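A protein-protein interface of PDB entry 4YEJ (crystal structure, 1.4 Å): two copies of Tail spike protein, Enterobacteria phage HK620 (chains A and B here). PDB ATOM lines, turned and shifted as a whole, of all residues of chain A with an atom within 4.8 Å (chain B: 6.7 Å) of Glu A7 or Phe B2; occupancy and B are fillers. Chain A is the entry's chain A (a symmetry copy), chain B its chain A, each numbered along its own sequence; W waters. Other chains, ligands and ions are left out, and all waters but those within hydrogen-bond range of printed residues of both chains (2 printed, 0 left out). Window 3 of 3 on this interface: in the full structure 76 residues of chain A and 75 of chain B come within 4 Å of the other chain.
NH1 of Arg A3 lies within hydrogen-bond range of OE1 of Gln B1. N of Gly B16 is in hydrogen-bond range of O of Ile A6 (3.0 Å).
The backbone carbonyl oxygen (O) of Ile A5 is in hydrogen-bond range of the side-chain hydroxyl (OG) of Ser A8, at 2.6 Å. NE of Arg A3 is in salt-bridge range of OE1 of Glu A7 (3.4 Å). N of Tyr B17 is in hydrogen-bond range of O of Arg B28. SD of Met B29 lies close to N of Val B15 (3.6 Å). N of Gly B16 sits at hydrogen-bond distance from SD of Met B29 (3.7 Å).
Among the printed residues, merely in contact across the chains: Ser A8 with Gly B16, Pro A9 with Tyr B17, Ile A6 with Val B15, Arg A3 with Phe B2, Glu A7 with His B14, Ile A6 with Phe B2, Pro A9 with Gly B16, Ile A6 with His B14, Glu A7 with Phe B2 and Glu A7 with Met B29.
Of chain B, only Phe B2, His B14 and Met B29 come within 4 Å of Glu A7. Phe B2 touches just these residues of chain A: Arg A3, Ile A6 and Glu A7. Of the printed residues of chain A, Tyr B17 touches Pro A9. Of the printed residues of chain B, Ser A8 touches Gly B16 (3.1 Å). Of the printed residues of chain A, Val B15 touches Ile A6. Ile B5 touches none of the printed residues of chain A. The nearest residue of chain B that does not touch Glu A7 is Gly B16 (4.2 Å). The nearest printed residue of chain A that does not touch Phe B2 is Ala A4 (5.9 Å). The nearest printed residue of chain A that does not touch Tyr B17 is Ser A8 (4.3 Å).
Of the 14 printed residues of chain B, 7 touch a printed residue of chain A. Hydrophobic or aromatic side chains of chain B that line the printed part of chain A: Phe B2, His B14, Val B15 and Met B29.
5 positions are printed for both chains. Of the 12 pairs that touch across the chains among the printed residues, none has its exchanged pair printed and touching as well.
Water W2 bridges the side-chain carboxylate (OE2) of Glu A7 (2.7 Å) and the backbone carbonyl oxygen (O) of His B14 (2.8 Å). Water W1 lies within hydrogen-bond range of NH1 of Arg A3 (2.9 Å) and OE1 of Gln B1 (3.4 Å).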
ATOM      1  N   ARG A   3      27.585 -14.381 -28.114  1.00  0.00           N
ATOM      2  CA  ARG A   3      26.491 -15.281 -27.719  1.00  0.00           C
ATOM      3  C   ARG A   3      26.541 -15.523 -26.214  1.00  0.00           C
ATOM      4  O   ARG A   3      25.503 -15.493 -25.561  1.00  0.00           O
ATOM      5  CB  ARG A   3      26.540 -16.645 -28.466  1.00  0.00           C
ATOM      6  CG  ARG A   3      25.621 -17.727 -27.824  1.00  0.00           C
ATOM      7  CD  ARG A   3      25.682 -19.117 -28.474  1.00  0.00           C
ATOM      8  NE  ARG A   3      24.380 -19.809 -28.480  1.00  0.00           N
ATOM      9  CZ  ARG A   3      24.095 -20.931 -29.167  1.00  0.00           C
ATOM     10  NH1 ARG A   3      25.021 -21.542 -29.933  1.00  0.00           N
ATOM     11  NH2 ARG A   3      22.842 -21.429 -29.130  1.00  0.00           N
ATOM     12  N   ALA A   4      27.727 -15.719 -25.646  1.00  0.00           N
ATOM     13  CA  ALA A   4      27.877 -15.975 -24.226  1.00  0.00           C
ATOM     14  C   ALA A   4      27.364 -14.759 -23.448  1.00  0.00           C
ATOM     15  O   ALA A   4      26.685 -14.936 -22.480  1.00  0.00           O
ATOM     16  CB  ALA A   4      29.305 -16.255 -23.829  1.00  0.00           C
ATOM     17  N   ILE A   5      27.745 -13.551 -23.876  1.00  0.00           N
ATOM     18  CA  ILE A   5      27.345 -12.288 -23.175  1.00  0.00           C
ATOM     19  C   ILE A   5      25.812 -12.204 -23.224  1.00  0.00           C
ATOM     20  O   ILE A   5      25.156 -11.963 -22.200  1.00  0.00           O
ATOM     21  CB  ILE A   5      28.011 -11.024 -23.833  1.00  0.00           C
ATOM     22  CG1 ILE A   5      29.527 -10.957 -23.516  1.00  0.00           C
ATOM     23  CG2 ILE A   5      27.338  -9.745 -23.433  1.00  0.00           C
ATOM     24  CD1 ILE A   5      30.412 -10.036 -24.418  1.00  0.00           C
ATOM     25  N   ILE A   6      25.244 -12.488 -24.400  1.00  0.00           N
ATOM     26  CA  ILE A   6      23.783 -12.353 -24.555  1.00  0.00           C
ATOM     27  C   ILE A   6      23.002 -13.297 -23.655  1.00  0.00           C
ATOM     28  O   ILE A   6      21.953 -12.888 -23.135  1.00  0.00           O
ATOM     29  CB  ILE A   6      23.405 -12.486 -26.052  1.00  0.00           C
ATOM     30  CG1 ILE A   6      23.946 -11.253 -26.796  1.00  0.00           C
ATOM     31  CG2 ILE A   6      21.865 -12.506 -26.263  1.00  0.00           C
ATOM     32  CD1 ILE A   6      23.229  -9.946 -26.589  1.00  0.00           C
ATOM     33  N   GLU A   7      23.480 -14.532 -23.498  1.00  0.00           N
ATOM     34  CA  GLU A   7      22.784 -15.508 -22.691  1.00  0.00           C
ATOM     35  C   GLU A   7      23.091 -15.338 -21.195  1.00  0.00           C
ATOM     36  O   GLU A   7      22.386 -15.902 -20.378  1.00  0.00           O
ATOM     37  CB  GLU A   7      23.090 -16.935 -23.173  1.00  0.00           C
ATOM     38  CG  GLU A   7      22.670 -17.186 -24.605  1.00  0.00           C
ATOM     39  CD  GLU A   7      22.495 -18.662 -24.923  1.00  0.00           C
ATOM     40  OE1 GLU A   7      23.499 -19.296 -25.241  1.00  0.00           O
ATOM     41  OE2 GLU A   7      21.322 -19.173 -24.868  1.00  0.00           O
ATOM     42  N   SER A   8      24.097 -14.525 -20.868  1.00  0.00           N
ATOM     43  CA  SER A   8      24.440 -14.247 -19.480  1.00  0.00           C
ATOM     44  C   SER A   8      23.469 -13.289 -18.849  1.00  0.00           C
ATOM     45  O   SER A   8      22.714 -12.623 -19.558  1.00  0.00           O
ATOM     46  CB  SER A   8      25.842 -13.626 -19.371  1.00  0.00           C
ATOM     47  OG  SER A   8      25.860 -12.252 -19.761  1.00  0.00           O
ATOM     48  N   PRO A   9      23.539 -13.133 -17.521  1.00  0.00           N
ATOM     49  CA  PRO A   9      22.659 -12.171 -16.863  1.00  0.00           C
ATOM     50  C   PRO A   9      22.909 -10.695 -17.268  1.00  0.00           C
ATOM     51  O   PRO A   9      22.068  -9.829 -17.009  1.00  0.00           O
ATOM     52  CB  PRO A   9      22.963 -12.353 -15.351  1.00  0.00           C
ATOM     53  CG  PRO A   9      23.536 -13.661 -15.241  1.00  0.00           C
ATOM     54  CD  PRO A   9      24.263 -13.956 -16.538  1.00  0.00           C
ATOM     55  N   GLN B   1      21.140 -20.486 -36.163  1.00  0.00           N
ATOM     56  CA  GLN B   1      21.579 -21.121 -34.904  1.00  0.00           C
ATOM     57  C   GLN B   1      21.077 -20.184 -33.792  1.00  0.00           C
ATOM     58  O   GLN B   1      19.887 -20.092 -33.504  1.00  0.00           O
ATOM     59  CB  GLN B   1      23.105 -21.299 -34.939  1.00  0.00           C
ATOM     60  CG  GLN B   1      23.770 -21.642 -33.595  1.00  0.00           C
ATOM     61  CD  GLN B   1      25.304 -21.689 -33.677  1.00  0.00           C
ATOM     62  OE1 GLN B   1      25.988 -21.790 -32.660  1.00  0.00           O
ATOM     63  NE2 GLN B   1      25.834 -21.607 -34.870  1.00  0.00           N
ATOM     64  N   PHE B   2      22.000 -19.443 -33.213  1.00  0.00           N
ATOM     65  CA  PHE B   2      21.684 -18.526 -32.172  1.00  0.00           C
ATOM     66  C   PHE B   2      20.924 -17.339 -32.767  1.00  0.00           C
ATOM     67  O   PHE B   2      19.946 -16.870 -32.187  1.00  0.00           O
ATOM     68  CB  PHE B   2      22.984 -18.024 -31.606  1.00  0.00           C
ATOM     69  CG  PHE B   2      22.800 -17.061 -30.491  1.00  0.00           C
ATOM     70  CD1 PHE B   2      22.067 -17.445 -29.359  1.00  0.00           C
ATOM     71  CD2 PHE B   2      23.346 -15.800 -30.556  1.00  0.00           C
ATOM     72  CE1 PHE B   2      21.898 -16.578 -28.320  1.00  0.00           C
ATOM     73  CE2 PHE B   2      23.222 -14.938 -29.495  1.00  0.00           C
ATOM     74  CZ  PHE B   2      22.499 -15.319 -28.393  1.00  0.00           C
ATOM     75  N   ARG B   3      21.386 -16.822 -33.897  1.00  0.00           N
ATOM     76  CA  ARG B   3      20.718 -15.687 -34.550  1.00  0.00           C
ATOM     77  C   ARG B   3      19.260 -16.035 -34.828  1.00  0.00           C
ATOM     78  O   ARG B   3      18.383 -15.211 -34.589  1.00  0.00           O
ATOM     79  CB  ARG B   3      21.413 -15.266 -35.876  1.00  0.00           C
ATOM     80  CG  ARG B   3      20.542 -14.315 -36.750  1.00  0.00           C
ATOM     81  CD  ARG B   3      21.146 -13.925 -38.107  1.00  0.00           C
ATOM     82  NE  ARG B   3      20.826 -12.542 -38.503  1.00  0.00           N
ATOM     83  CZ  ARG B   3      21.393 -11.870 -39.524  1.00  0.00           C
ATOM     84  NH1 ARG B   3      22.335 -12.438 -40.304  1.00  0.00           N
ATOM     85  NH2 ARG B   3      21.048 -10.584 -39.742  1.00  0.00           N
ATOM     86  N   ALA B   4      18.978 -17.252 -35.286  1.00  0.00           N
ATOM     87  CA  ALA B   4      17.626 -17.673 -35.596  1.00  0.00           C
ATOM     88  C   ALA B   4      16.787 -17.628 -34.316  1.00  0.00           C
ATOM     89  O   ALA B   4      15.682 -17.174 -34.364  1.00  0.00           O
ATOM     90  CB  ALA B   4      17.566 -19.061 -36.185  1.00  0.00           C
ATOM     91  N   ILE B   5      17.330 -18.146 -33.209  1.00  0.00           N
ATOM     92  CA  ILE B   5      16.593 -18.200 -31.904  1.00  0.00           C
ATOM     93  C   ILE B   5      16.285 -16.754 -31.493  1.00  0.00           C
ATOM     94  O   ILE B   5      15.143 -16.423 -31.139  1.00  0.00           O
ATOM     95  CB  ILE B   5      17.427 -18.947 -30.798  1.00  0.00           C
ATOM     96  CG1 ILE B   5      17.476 -20.473 -31.064  1.00  0.00           C
ATOM     97  CG2 ILE B   5      16.920 -18.676 -29.414  1.00  0.00           C
ATOM     98  CD1 ILE B   5      18.587 -21.297 -30.336  1.00  0.00           C
ATOM     99  N   ILE B   6      17.287 -15.878 -31.624  1.00  0.00           N
ATOM    100  CA  ILE B   6      17.100 -14.484 -31.177  1.00  0.00           C
ATOM    101  C   ILE B   6      16.014 -13.754 -31.950  1.00  0.00           C
ATOM    102  O   ILE B   6      15.275 -12.968 -31.336  1.00  0.00           O
ATOM    103  CB  ILE B   6      18.461 -13.746 -31.194  1.00  0.00           C
ATOM    104  CG1 ILE B   6      19.349 -14.347 -30.090  1.00  0.00           C
ATOM    105  CG2 ILE B   6      18.306 -12.232 -30.879  1.00  0.00           C
ATOM    106  CD1 ILE B   6      19.020 -13.994 -28.665  1.00  0.00           C
ATOM    107  N   GLU B   7      15.934 -13.981 -33.261  1.00  0.00           N
ATOM    108  CA  GLU B   7      14.958 -13.303 -34.082  1.00  0.00           C
ATOM    109  C   GLU B   7      13.582 -13.982 -34.012  1.00  0.00           C
ATOM    110  O   GLU B   7      12.605 -13.385 -34.430  1.00  0.00           O
ATOM    111  CB  GLU B   7      15.455 -13.175 -35.532  1.00  0.00           C
ATOM    112  CG  GLU B   7      16.740 -12.387 -35.657  1.00  0.00           C
ATOM    113  CD  GLU B   7      16.963 -11.833 -37.053  1.00  0.00           C
ATOM    114  OE1 GLU B   7      17.488 -12.576 -37.882  1.00  0.00           O
ATOM    115  OE2 GLU B   7      16.620 -10.624 -37.302  1.00  0.00           O
ATOM    116  N   GLY B  13      13.372 -14.793 -24.583  1.00  0.00           N
ATOM    117  CA  GLY B  13      13.571 -15.902 -23.677  1.00  0.00           C
ATOM    118  C   GLY B  13      14.982 -16.464 -23.606  1.00  0.00           C
ATOM    119  O   GLY B  13      15.213 -17.412 -22.872  1.00  0.00           O
ATOM    120  N   HIS B  14      15.877 -15.869 -24.395  1.00  0.00           N
ATOM    121  CA  HIS B  14      17.280 -16.302 -24.411  1.00  0.00           C
ATOM    122  C   HIS B  14      18.249 -15.211 -23.956  1.00  0.00           C
ATOM    123  O   HIS B  14      19.461 -15.476 -23.908  1.00  0.00           O
ATOM    124  CB  HIS B  14      17.656 -16.839 -25.794  1.00  0.00           C
ATOM    125  CG  HIS B  14      17.057 -18.177 -26.043  1.00  0.00           C
ATOM    126  ND1 HIS B  14      15.729 -18.329 -26.368  1.00  0.00           N
ATOM    127  CD2 HIS B  14      17.575 -19.423 -25.956  1.00  0.00           C
ATOM    128  CE1 HIS B  14      15.463 -19.611 -26.520  1.00  0.00           C
ATOM    129  NE2 HIS B  14      16.559 -20.297 -26.238  1.00  0.00           N
ATOM    130  N   VAL B  15      17.752 -14.000 -23.745  1.00  0.00           N
ATOM    131  CA  VAL B  15      18.560 -12.872 -23.422  1.00  0.00           C
ATOM    132  C   VAL B  15      18.500 -12.665 -21.908  1.00  0.00           C
ATOM    133  O   VAL B  15      17.438 -12.415 -21.344  1.00  0.00           O
ATOM    134  CB  VAL B  15      18.085 -11.587 -24.123  1.00  0.00           C
ATOM    135  CG1 VAL B  15      18.962 -10.414 -23.739  1.00  0.00           C
ATOM    136  CG2 VAL B  15      18.025 -11.711 -25.634  1.00  0.00           C
ATOM    137  N   GLY B  16      19.643 -12.809 -21.243  1.00  0.00           N
ATOM    138  CA  GLY B  16      19.654 -12.806 -19.759  1.00  0.00           C
ATOM    139  C   GLY B  16      19.477 -11.416 -19.195  1.00  0.00           C
ATOM    140  O   GLY B  16      19.855 -10.385 -19.840  1.00  0.00           O
ATOM    141  N   TYR B  17      18.960 -11.391 -17.973  1.00  0.00           N
ATOM    142  CA  TYR B  17      18.762 -10.158 -17.229  1.00  0.00           C
ATOM    143  C   TYR B  17      18.860 -10.384 -15.746  1.00  0.00           C
ATOM    144  O   TYR B  17      18.381 -11.417 -15.219  1.00  0.00           O
ATOM    145  CB  TYR B  17      17.393  -9.599 -17.590  1.00  0.00           C
ATOM    146  CG  TYR B  17      16.957  -8.392 -16.759  1.00  0.00           C
ATOM    147  CD1 TYR B  17      17.519  -7.104 -16.908  1.00  0.00           C
ATOM    148  CD2 TYR B  17      16.038  -8.563 -15.765  1.00  0.00           C
ATOM    149  CE1 TYR B  17      17.109  -6.044 -16.100  1.00  0.00           C
ATOM    150  CE2 TYR B  17      15.603  -7.518 -14.947  1.00  0.00           C
ATOM    151  CZ  TYR B  17      16.129  -6.257 -15.134  1.00  0.00           C
ATOM    152  OH  TYR B  17      15.686  -5.191 -14.375  1.00  0.00           O
ATOM    153  N   ARG B  28      17.226 -13.945 -14.629  1.00  0.00           N
ATOM    154  CA  ARG B  28      16.020 -14.075 -15.429  1.00  0.00           C
ATOM    155  C   ARG B  28      16.374 -13.946 -16.894  1.00  0.00           C
ATOM    156  O   ARG B  28      17.537 -13.736 -17.274  1.00  0.00           O
ATOM    157  CB  ARG B  28      15.026 -12.943 -15.044  1.00  0.00           C
ATOM    158  CG  ARG B  28      14.774 -12.807 -13.534  1.00  0.00           C
ATOM    159  CD  ARG B  28      13.814 -11.672 -13.269  1.00  0.00           C
ATOM    160  NE  ARG B  28      12.449 -12.076 -13.554  1.00  0.00           N
ATOM    161  CZ  ARG B  28      11.394 -11.262 -13.449  1.00  0.00           C
ATOM    162  NH1 ARG B  28      11.572  -9.972 -13.052  1.00  0.00           N
ATOM    163  NH2 ARG B  28      10.191 -11.729 -13.729  1.00  0.00           N
ATOM    164  N   MET B  29      15.337 -14.086 -17.703  1.00  0.00           N
ATOM    165  CA  MET B  29      15.393 -13.727 -19.144  1.00  0.00           C
ATOM    166  C   MET B  29      14.500 -12.500 -19.412  1.00  0.00           C
ATOM    167  O   MET B  29      13.559 -12.210 -18.684  1.00  0.00           O
ATOM    168  CB  MET B  29      14.981 -14.910 -20.049  1.00  0.00           C
ATOM    169  CG  MET B  29      15.907 -16.102 -19.908  1.00  0.00           C
ATOM    170  SD  MET B  29      17.496 -15.793 -20.679  1.00  0.00           S
ATOM    171  CE  MET B  29      18.626 -16.696 -19.620  1.00  0.00           C
HETATM  172  O   HOH W   1      23.957 -23.959 -31.027  1.00  0.00           O
HETATM  173  O   HOH W   2      19.724 -18.047 -22.936  1.00  0.00           O
